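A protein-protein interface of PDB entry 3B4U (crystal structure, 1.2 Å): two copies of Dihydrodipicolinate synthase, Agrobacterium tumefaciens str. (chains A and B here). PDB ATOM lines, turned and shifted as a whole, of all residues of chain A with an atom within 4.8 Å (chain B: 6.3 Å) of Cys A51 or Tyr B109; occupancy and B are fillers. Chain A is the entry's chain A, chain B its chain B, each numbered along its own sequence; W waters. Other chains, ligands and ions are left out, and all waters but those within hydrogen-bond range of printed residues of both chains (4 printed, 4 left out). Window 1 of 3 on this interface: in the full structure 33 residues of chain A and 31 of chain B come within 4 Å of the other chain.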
ATOM      1  N   THR A  46      27.835 -19.067  -1.406  1.00  0.00           N
ATOM      2  CA  THR A  46      28.613 -18.460  -2.490  1.00  0.00           C
ATOM      3  C   THR A  46      30.112 -18.732  -2.321  1.00  0.00           C
ATOM      4  O   THR A  46      30.784 -19.139  -3.273  1.00  0.00           O
ATOM      5  CB  THR A  46      28.322 -16.958  -2.577  1.00  0.00           C
ATOM      6  OG1 THR A  46      26.907 -16.782  -2.774  1.00  0.00           O
ATOM      7  CG2 THR A  46      29.101 -16.285  -3.678  1.00  0.00           C
ATOM      8  N   GLU A  49      31.321 -22.070  -3.245  1.00  0.00           N
ATOM      9  CA  GLU A  49      31.084 -22.489  -4.617  1.00  0.00           C
ATOM     10  C   GLU A  49      29.888 -23.439  -4.695  1.00  0.00           C
ATOM     11  O   GLU A  49      29.855 -24.368  -5.482  1.00  0.00           O
ATOM     12  CB  GLU A  49      32.352 -23.096  -5.269  1.00  0.00           C
ATOM     13  CG  GLU A  49      33.506 -22.105  -5.358  1.00  0.00           C
ATOM     14  CD  GLU A  49      34.814 -22.766  -5.671  1.00  0.00           C
ATOM     15  OE1 GLU A  49      34.983 -23.207  -6.829  1.00  0.00           O
ATOM     16  OE2 GLU A  49      35.665 -22.883  -4.748  1.00  0.00           O
ATOM     17  N   GLY A  50      28.851 -23.154  -3.910  1.00  0.00           N
ATOM     18  CA  GLY A  50      27.717 -24.061  -3.800  1.00  0.00           C
ATOM     19  C   GLY A  50      27.025 -24.274  -5.130  1.00  0.00           C
ATOM     20  O   GLY A  50      26.559 -25.364  -5.433  1.00  0.00           O
ATOM     21  N   CYS A  51      26.987 -23.221  -5.951  1.00  0.00           N
ATOM     22  CA  CYS A  51      26.405 -23.341  -7.283  1.00  0.00           C
ATOM     23  C   CYS A  51      27.108 -24.379  -8.137  1.00  0.00           C
ATOM     24  O   CYS A  51      26.495 -24.988  -9.015  1.00  0.00           O
ATOM     25  CB  CYS A  51      26.453 -21.975  -7.981  1.00  0.00           C
ATOM     26  SG  CYS A  51      28.089 -21.164  -7.937  1.00  0.00           S
ATOM     27  N   SER A  52      28.382 -24.622  -7.830  1.00  0.00           N
ATOM     28  CA  SER A  52      29.209 -25.560  -8.592  1.00  0.00           C
ATOM     29  C   SER A  52      29.219 -26.953  -7.978  1.00  0.00           C
ATOM     30  O   SER A  52      29.798 -27.869  -8.566  1.00  0.00           O
ATOM     31  CB  SER A  52      30.624 -25.037  -8.659  1.00  0.00           C
ATOM     32  OG  SER A  52      30.618 -23.730  -9.188  1.00  0.00           O
ATOM     33  N   VAL A  53      28.587 -27.122  -6.820  1.00  0.00           N
ATOM     34  CA  VAL A  53      28.506 -28.409  -6.148  1.00  0.00           C
ATOM     35  C   VAL A  53      27.250 -29.095  -6.636  1.00  0.00           C
ATOM     36  O   VAL A  53      26.147 -28.553  -6.581  1.00  0.00           O
ATOM     37  CB  VAL A  53      28.520 -28.230  -4.631  1.00  0.00           C
ATOM     38  CG1 VAL A  53      28.295 -29.569  -3.936  1.00  0.00           C
ATOM     39  CG2 VAL A  53      29.850 -27.609  -4.227  1.00  0.00           C
ATOM     40  N   LEU A  80      20.649 -22.762  -3.736  1.00  0.00           N
ATOM     41  CA  LEU A  80      20.957 -21.745  -4.744  1.00  0.00           C
ATOM     42  C   LEU A  80      20.416 -22.174  -6.103  1.00  0.00           C
ATOM     43  O   LEU A  80      21.075 -22.019  -7.126  1.00  0.00           O
ATOM     44  CB  LEU A  80      22.476 -21.515  -4.857  1.00  0.00           C
ATOM     45  CG  LEU A  80      23.282 -21.225  -3.587  1.00  0.00           C
ATOM     46  CD1 LEU A  80      24.766 -21.110  -3.904  1.00  0.00           C
ATOM     47  CD2 LEU A  80      22.779 -19.989  -2.828  1.00  0.00           C
ATOM     48  N   SER A 108      17.558 -17.424  -9.820  1.00  0.00           N
ATOM     49  CA  SER A 108      18.563 -16.516 -10.369  1.00  0.00           C
ATOM     50  C   SER A 108      18.824 -16.723 -11.860  1.00  0.00           C
ATOM     51  O   SER A 108      19.883 -16.338 -12.364  1.00  0.00           O
ATOM     52  CB  SER A 108      19.866 -16.623  -9.538  1.00  0.00           C
ATOM     53  OG  SER A 108      20.451 -17.901  -9.644  1.00  0.00           O
ATOM     54  N   TYR A 139      18.365 -15.110   1.188  1.00  0.00           N
ATOM     55  CA  TYR A 139      19.687 -14.648   0.820  1.00  0.00           C
ATOM     56  C   TYR A 139      19.611 -13.490  -0.173  1.00  0.00           C
ATOM     57  O   TYR A 139      19.222 -13.678  -1.327  1.00  0.00           O
ATOM     58  CB  TYR A 139      20.453 -15.827   0.247  1.00  0.00           C
ATOM     59  CG  TYR A 139      21.947 -15.717   0.083  1.00  0.00           C
ATOM     60  CD1 TYR A 139      22.712 -14.668   0.602  1.00  0.00           C
ATOM     61  CD2 TYR A 139      22.619 -16.714  -0.590  1.00  0.00           C
ATOM     62  CE1 TYR A 139      24.094 -14.627   0.441  1.00  0.00           C
ATOM     63  CE2 TYR A 139      24.014 -16.692  -0.726  1.00  0.00           C
ATOM     64  CZ  TYR A 139      24.726 -15.645  -0.223  1.00  0.00           C
ATOM     65  OH  TYR A 139      26.097 -15.644  -0.376  1.00  0.00           O
ATOM     66  N   ILE A 141      21.779 -11.242  -2.184  1.00  0.00           N
ATOM     67  CA  ILE A 141      23.132 -11.039  -2.715  1.00  0.00           C
ATOM     68  C   ILE A 141      23.012 -10.599  -4.176  1.00  0.00           C
ATOM     69  O   ILE A 141      23.400 -11.292  -5.123  1.00  0.00           O
ATOM     70  CB  ILE A 141      24.023 -12.283  -2.488  1.00  0.00           C
ATOM     71  CG1 ILE A 141      25.473 -11.957  -2.884  1.00  0.00           C
ATOM     72  CG2 ILE A 141      23.467 -13.553  -3.157  1.00  0.00           C
ATOM     73  CD1 ILE A 141      26.460 -13.046  -2.507  1.00  0.00           C
ATOM     74  N   VAL A 144      25.490 -10.991  -7.149  1.00  0.00           N
ATOM     75  CA  VAL A 144      25.654 -12.304  -7.744  1.00  0.00           C
ATOM     76  C   VAL A 144      24.356 -12.750  -8.412  1.00  0.00           C
ATOM     77  O   VAL A 144      24.357 -13.114  -9.579  1.00  0.00           O
ATOM     78  CB  VAL A 144      26.128 -13.315  -6.696  1.00  0.00           C
ATOM     79  CG1 VAL A 144      26.225 -14.686  -7.334  1.00  0.00           C
ATOM     80  CG2 VAL A 144      27.463 -12.883  -6.101  1.00  0.00           C
ATOM     81  N   THR A 145      23.226 -12.745  -7.704  1.00  0.00           N
ATOM     82  CA  THR A 145      21.992 -13.245  -8.273  1.00  0.00           C
ATOM     83  C   THR A 145      21.276 -12.266  -9.193  1.00  0.00           C
ATOM     84  O   THR A 145      20.418 -12.683  -9.962  1.00  0.00           O
ATOM     85  CB  THR A 145      20.975 -13.643  -7.185  1.00  0.00           C
ATOM     86  OG1 THR A 145      20.728 -12.465  -6.420  1.00  0.00           O
ATOM     87  CG2 THR A 145      21.478 -14.759  -6.316  1.00  0.00           C
ATOM     88  N   VAL B  81      21.551 -25.262 -15.859  1.00  0.00           N
ATOM     89  CA  VAL B  81      22.031 -25.425 -14.470  1.00  0.00           C
ATOM     90  C   VAL B  81      23.461 -24.931 -14.302  1.00  0.00           C
ATOM     91  O   VAL B  81      24.137 -24.488 -15.258  1.00  0.00           O
ATOM     92  CB  VAL B  81      21.871 -26.870 -13.992  1.00  0.00           C
ATOM     93  CG1 VAL B  81      20.388 -27.233 -13.985  1.00  0.00           C
ATOM     94  CG2 VAL B  81      22.687 -27.805 -14.862  1.00  0.00           C
ATOM     95  N   ASP B  82      23.925 -24.948 -13.064  1.00  0.00           N
ATOM     96  CA  ASP B  82      25.174 -24.257 -12.743  1.00  0.00           C
ATOM     97  C   ASP B  82      26.313 -25.172 -12.347  1.00  0.00           C
ATOM     98  O   ASP B  82      27.450 -24.718 -12.254  1.00  0.00           O
ATOM     99  CB  ASP B  82      24.925 -23.202 -11.675  1.00  0.00           C
ATOM    100  CG  ASP B  82      23.758 -22.319 -12.060  1.00  0.00           C
ATOM    101  OD1 ASP B  82      23.734 -21.899 -13.247  1.00  0.00           O
ATOM    102  OD2 ASP B  82      22.872 -22.087 -11.217  1.00  0.00           O
ATOM    103  N   SER B  83      26.045 -26.447 -12.124  1.00  0.00           N
ATOM    104  CA  SER B  83      27.084 -27.381 -11.726  1.00  0.00           C
ATOM    105  C   SER B  83      27.384 -28.322 -12.862  1.00  0.00           C
ATOM    106  O   SER B  83      26.519 -28.691 -13.679  1.00  0.00           O
ATOM    107  CB  SER B  83      26.651 -28.181 -10.481  1.00  0.00           C
ATOM    108  OG  SER B  83      25.538 -29.011 -10.771  1.00  0.00           O
ATOM    109  N   ILE B  84      28.639 -28.778 -12.883  1.00  0.00           N
ATOM    110  CA  ILE B  84      29.088 -29.769 -13.833  1.00  0.00           C
ATOM    111  C   ILE B  84      28.272 -31.044 -13.677  1.00  0.00           C
ATOM    112  O   ILE B  84      27.840 -31.636 -14.678  1.00  0.00           O
ATOM    113  CB  ILE B  84      30.610 -30.030 -13.624  1.00  0.00           C
ATOM    114  CG1 ILE B  84      31.414 -28.791 -14.066  1.00  0.00           C
ATOM    115  CG2 ILE B  84      31.056 -31.295 -14.367  1.00  0.00           C
ATOM    116  CD1 ILE B  84      32.801 -28.704 -13.423  1.00  0.00           C
ATOM    117  N   PRO B 107      26.918 -22.024 -17.026  1.00  0.00           N
ATOM    118  CA  PRO B 107      26.462 -21.779 -15.679  1.00  0.00           C
ATOM    119  C   PRO B 107      26.201 -20.277 -15.468  1.00  0.00           C
ATOM    120  O   PRO B 107      26.897 -19.438 -16.043  1.00  0.00           O
ATOM    121  CB  PRO B 107      27.626 -22.312 -14.848  1.00  0.00           C
ATOM    122  CG  PRO B 107      28.845 -22.119 -15.729  1.00  0.00           C
ATOM    123  CD  PRO B 107      28.329 -22.441 -17.073  1.00  0.00           C
ATOM    124  N   SER B 108      25.211 -19.944 -14.639  1.00  0.00           N
ATOM    125  CA  SER B 108      24.629 -18.608 -14.599  1.00  0.00           C
ATOM    126  C   SER B 108      24.445 -18.064 -13.188  1.00  0.00           C
ATOM    127  O   SER B 108      23.610 -17.176 -12.972  1.00  0.00           O
ATOM    128  CB  SER B 108      23.304 -18.601 -15.393  1.00  0.00           C
ATOM    129  OG  SER B 108      22.304 -19.433 -14.833  1.00  0.00           O
ATOM    130  N   TYR B 109      25.213 -18.572 -12.238  1.00  0.00           N
ATOM    131  CA  TYR B 109      25.208 -18.020 -10.882  1.00  0.00           C
ATOM    132  C   TYR B 109      26.357 -17.019 -10.715  1.00  0.00           C
ATOM    133  O   TYR B 109      26.134 -15.813 -10.571  1.00  0.00           O
ATOM    134  CB  TYR B 109      25.232 -19.159  -9.855  1.00  0.00           C
ATOM    135  CG  TYR B 109      25.068 -18.687  -8.426  1.00  0.00           C
ATOM    136  CD1 TYR B 109      23.817 -18.489  -7.840  1.00  0.00           C
ATOM    137  CD2 TYR B 109      26.169 -18.398  -7.643  1.00  0.00           C
ATOM    138  CE1 TYR B 109      23.705 -18.066  -6.525  1.00  0.00           C
ATOM    139  CE2 TYR B 109      26.049 -17.957  -6.329  1.00  0.00           C
ATOM    140  CZ  TYR B 109      24.832 -17.790  -5.787  1.00  0.00           C
ATOM    141  OH  TYR B 109      24.690 -17.356  -4.468  1.00  0.00           O
ATOM    142  N   PHE B 110      27.596 -17.484 -10.789  1.00  0.00           N
ATOM    143  CA  PHE B 110      28.744 -16.596 -10.781  1.00  0.00           C
ATOM    144  C   PHE B 110      28.692 -15.683 -11.993  1.00  0.00           C
ATOM    145  O   PHE B 110      28.331 -16.097 -13.093  1.00  0.00           O
ATOM    146  CB  PHE B 110      30.071 -17.366 -10.735  1.00  0.00           C
ATOM    147  CG  PHE B 110      30.382 -18.011  -9.385  1.00  0.00           C
ATOM    148  CD1 PHE B 110      30.300 -17.295  -8.210  1.00  0.00           C
ATOM    149  CD2 PHE B 110      30.787 -19.334  -9.317  1.00  0.00           C
ATOM    150  CE1 PHE B 110      30.623 -17.901  -6.997  1.00  0.00           C
ATOM    151  CE2 PHE B 110      31.120 -19.914  -8.111  1.00  0.00           C
ATOM    152  CZ  PHE B 110      31.039 -19.202  -6.953  1.00  0.00           C
ATOM    153  N   LYS B 111      29.087 -14.441 -11.781  1.00  0.00           N
ATOM    154  CA  LYS B 111      29.088 -13.389 -12.786  1.00  0.00           C
ATOM    155  C   LYS B 111      30.496 -13.041 -13.248  1.00  0.00           C
ATOM    156  O   LYS B 111      31.468 -13.325 -12.573  1.00  0.00           O
ATOM    157  CB  LYS B 111      28.429 -12.139 -12.194  1.00  0.00           C
ATOM    158  CG  LYS B 111      26.966 -12.355 -11.771  1.00  0.00           C
ATOM    159  CD  LYS B 111      26.063 -12.432 -12.970  1.00  0.00           C
ATOM    160  CE  LYS B 111      24.607 -12.818 -12.632  1.00  0.00           C
ATOM    161  NZ  LYS B 111      24.462 -14.241 -12.172  1.00  0.00           N
ATOM    162  N   THR B 145      21.484 -14.899 -19.013  1.00  0.00           N
ATOM    163  CA  THR B 145      22.476 -15.538 -18.167  1.00  0.00           C
ATOM    164  C   THR B 145      23.580 -14.584 -17.681  1.00  0.00           C
ATOM    165  O   THR B 145      24.291 -14.906 -16.758  1.00  0.00           O
ATOM    166  CB  THR B 145      23.168 -16.686 -18.900  1.00  0.00           C
ATOM    167  OG1 THR B 145      23.803 -16.119 -20.046  1.00  0.00           O
ATOM    168  CG2 THR B 145      22.213 -17.799 -19.292  1.00  0.00           C
ATOM    169  N   VAL B 147      26.179 -14.292 -19.331  1.00  0.00           N
ATOM    170  CA  VAL B 147      27.376 -15.010 -19.766  1.00  0.00           C
ATOM    171  C   VAL B 147      27.360 -15.053 -21.288  1.00  0.00           C
ATOM    172  O   VAL B 147      26.519 -15.662 -21.918  1.00  0.00           O
ATOM    173  CB  VAL B 147      27.450 -16.414 -19.160  1.00  0.00           C
ATOM    174  CG1 VAL B 147      28.735 -17.074 -19.636  1.00  0.00           C
ATOM    175  CG2 VAL B 147      27.366 -16.356 -17.630  1.00  0.00           C
HETATM  176  O   HOH W   1      29.317 -30.415 -10.062  1.00  0.00           O
HETATM  177  O   HOH W   2      24.167 -28.449  -8.549  1.00  0.00           O
HETATM  178  O   HOH W   3      28.875 -22.592 -11.278  1.00  0.00           O
HETATM  179  O   HOH W   4      21.687 -14.418 -11.751  1.00  0.00           O
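Among the printed residues, merely in contact across the chains: Thr A46 with Phe B110, Cys A51 with Tyr B109, Cys A51 with Phe B110, Ser A52 with Ser B83, Ser A52 with Phe B110, Val A53 with Ser B83, Leu A80 with Tyr B109, Ser A108 with Ser B108, Ser A108 with Tyr B109, Tyr A139 with Tyr B109 and Thr A145 with Tyr B109.
Water W2 bridges the side-chain hydroxyl of Ser B83 (2.7 Å) and the backbone carbonyl oxygen of Val A53 (2.8 Å). Water W4 lies within hydrogen-bond range of O of Ser A108, O of Thr A145 and NZ of Lys B111. Water W3 lies within hydrogen-bond range of the backbone carbonyl oxygen of Asp B82, the side-chain hydroxyl of Ser A52 and the side-chain sulfur of Cys A51. Water W1 lies within hydrogen-bond range of the backbone carbonyl oxygen (O) of Ser A52 (3.0 Å) and the backbone NH (N) of Ile B84 (3.3 Å).
Ser A108 touches its own counterpart, Ser B108. Positions printed for both chains: 108 and 145.
The side-chain hydroxyl (OG1) of Thr A46 sits at hydrogen-bond distance from the side-chain hydroxyl (OH) of Tyr A139. The backbone carbonyl oxygen (O) of Ile A141 lies within hydrogen-bond range of the side-chain hydroxyl (OG1) of Thr A145. N of Ser B108 sits at hydrogen-bond distance from OD1 of Asp B82, at 2.8 Å. O of Ser B108 is in hydrogen-bond range of NZ of Lys B111, at 3.2 Å. The backbone carbonyl oxygen of Tyr B109 is in hydrogen-bond range of the side-chain amino group of Lys B111 (2.8 Å).
Of the printed residues of chain A, Tyr B109 touches Thr A46, Cys A51, Leu A80, Ser A108, Tyr A139, Val A144 and Thr A145. Of the printed residues of chain A, Phe B110 touches Thr A46 (3.7 Å), Cys A51 (3.3 Å) and Ser A52 (3.997 Å). Of the printed residues of chain A, Asp B82 touches Cys A51 (3.3 Å). Printed residues of chain A within 4 Å of Ser B83: Cys A51 (3.5 Å), Ser A52 (3.7 Å) and Val A53 (3.9 Å). Printed residues of chain B within 4 Å of Ser A108: Ser B108 and Tyr B109. Pro B107 touches none of the printed residues of chain A. Glu A49 touches none of the printed residues of chain B. The nearest residue of chain B that does not touch Cys A51 is Ile B84 (5.8 Å). The nearest printed residue of chain A that does not touch Ser B83 is Gly A50 (5.8 Å).
OG1 of Thr A46 is in hydrogen-bond range of OH of Tyr B109 (2.8 Å). O of Cys A51 sits at hydrogen-bond distance from N of Ser B83, 3.5 Å away. The backbone carbonyl oxygen (O) of Val A144 lies within hydrogen-bond range of the side-chain amino group (NZ) of Lys B111 (2.8 Å). The backbone carbonyl oxygen of Cys A51 lies close to the backbone carbonyl oxygen of Asp B82, at 3.4 Å. O of Tyr B109 lies close to O of Val A144, 3.4 Å away.
Of the 11 printed residues of chain B, 6 touch a printed residue of chain A. Hydrophobic or aromatic side chains of chain B within 4 Å of the printed part of chain A: Tyr B109 and Phe B110. Of the 12 printed residues of chain A, 9 touch a printed residue of chain B. Hydrophobic or aromatic side chains of chain A that line the printed part of chain B: Leu A80, Tyr A139 and Val A144. Among the printed residues, 16 pairs touch across the chains. Among the printed residues, no Asp or Glu carboxylate lies within 4 Å of a Lys or Arg side-chain nitrogen of the other chain.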
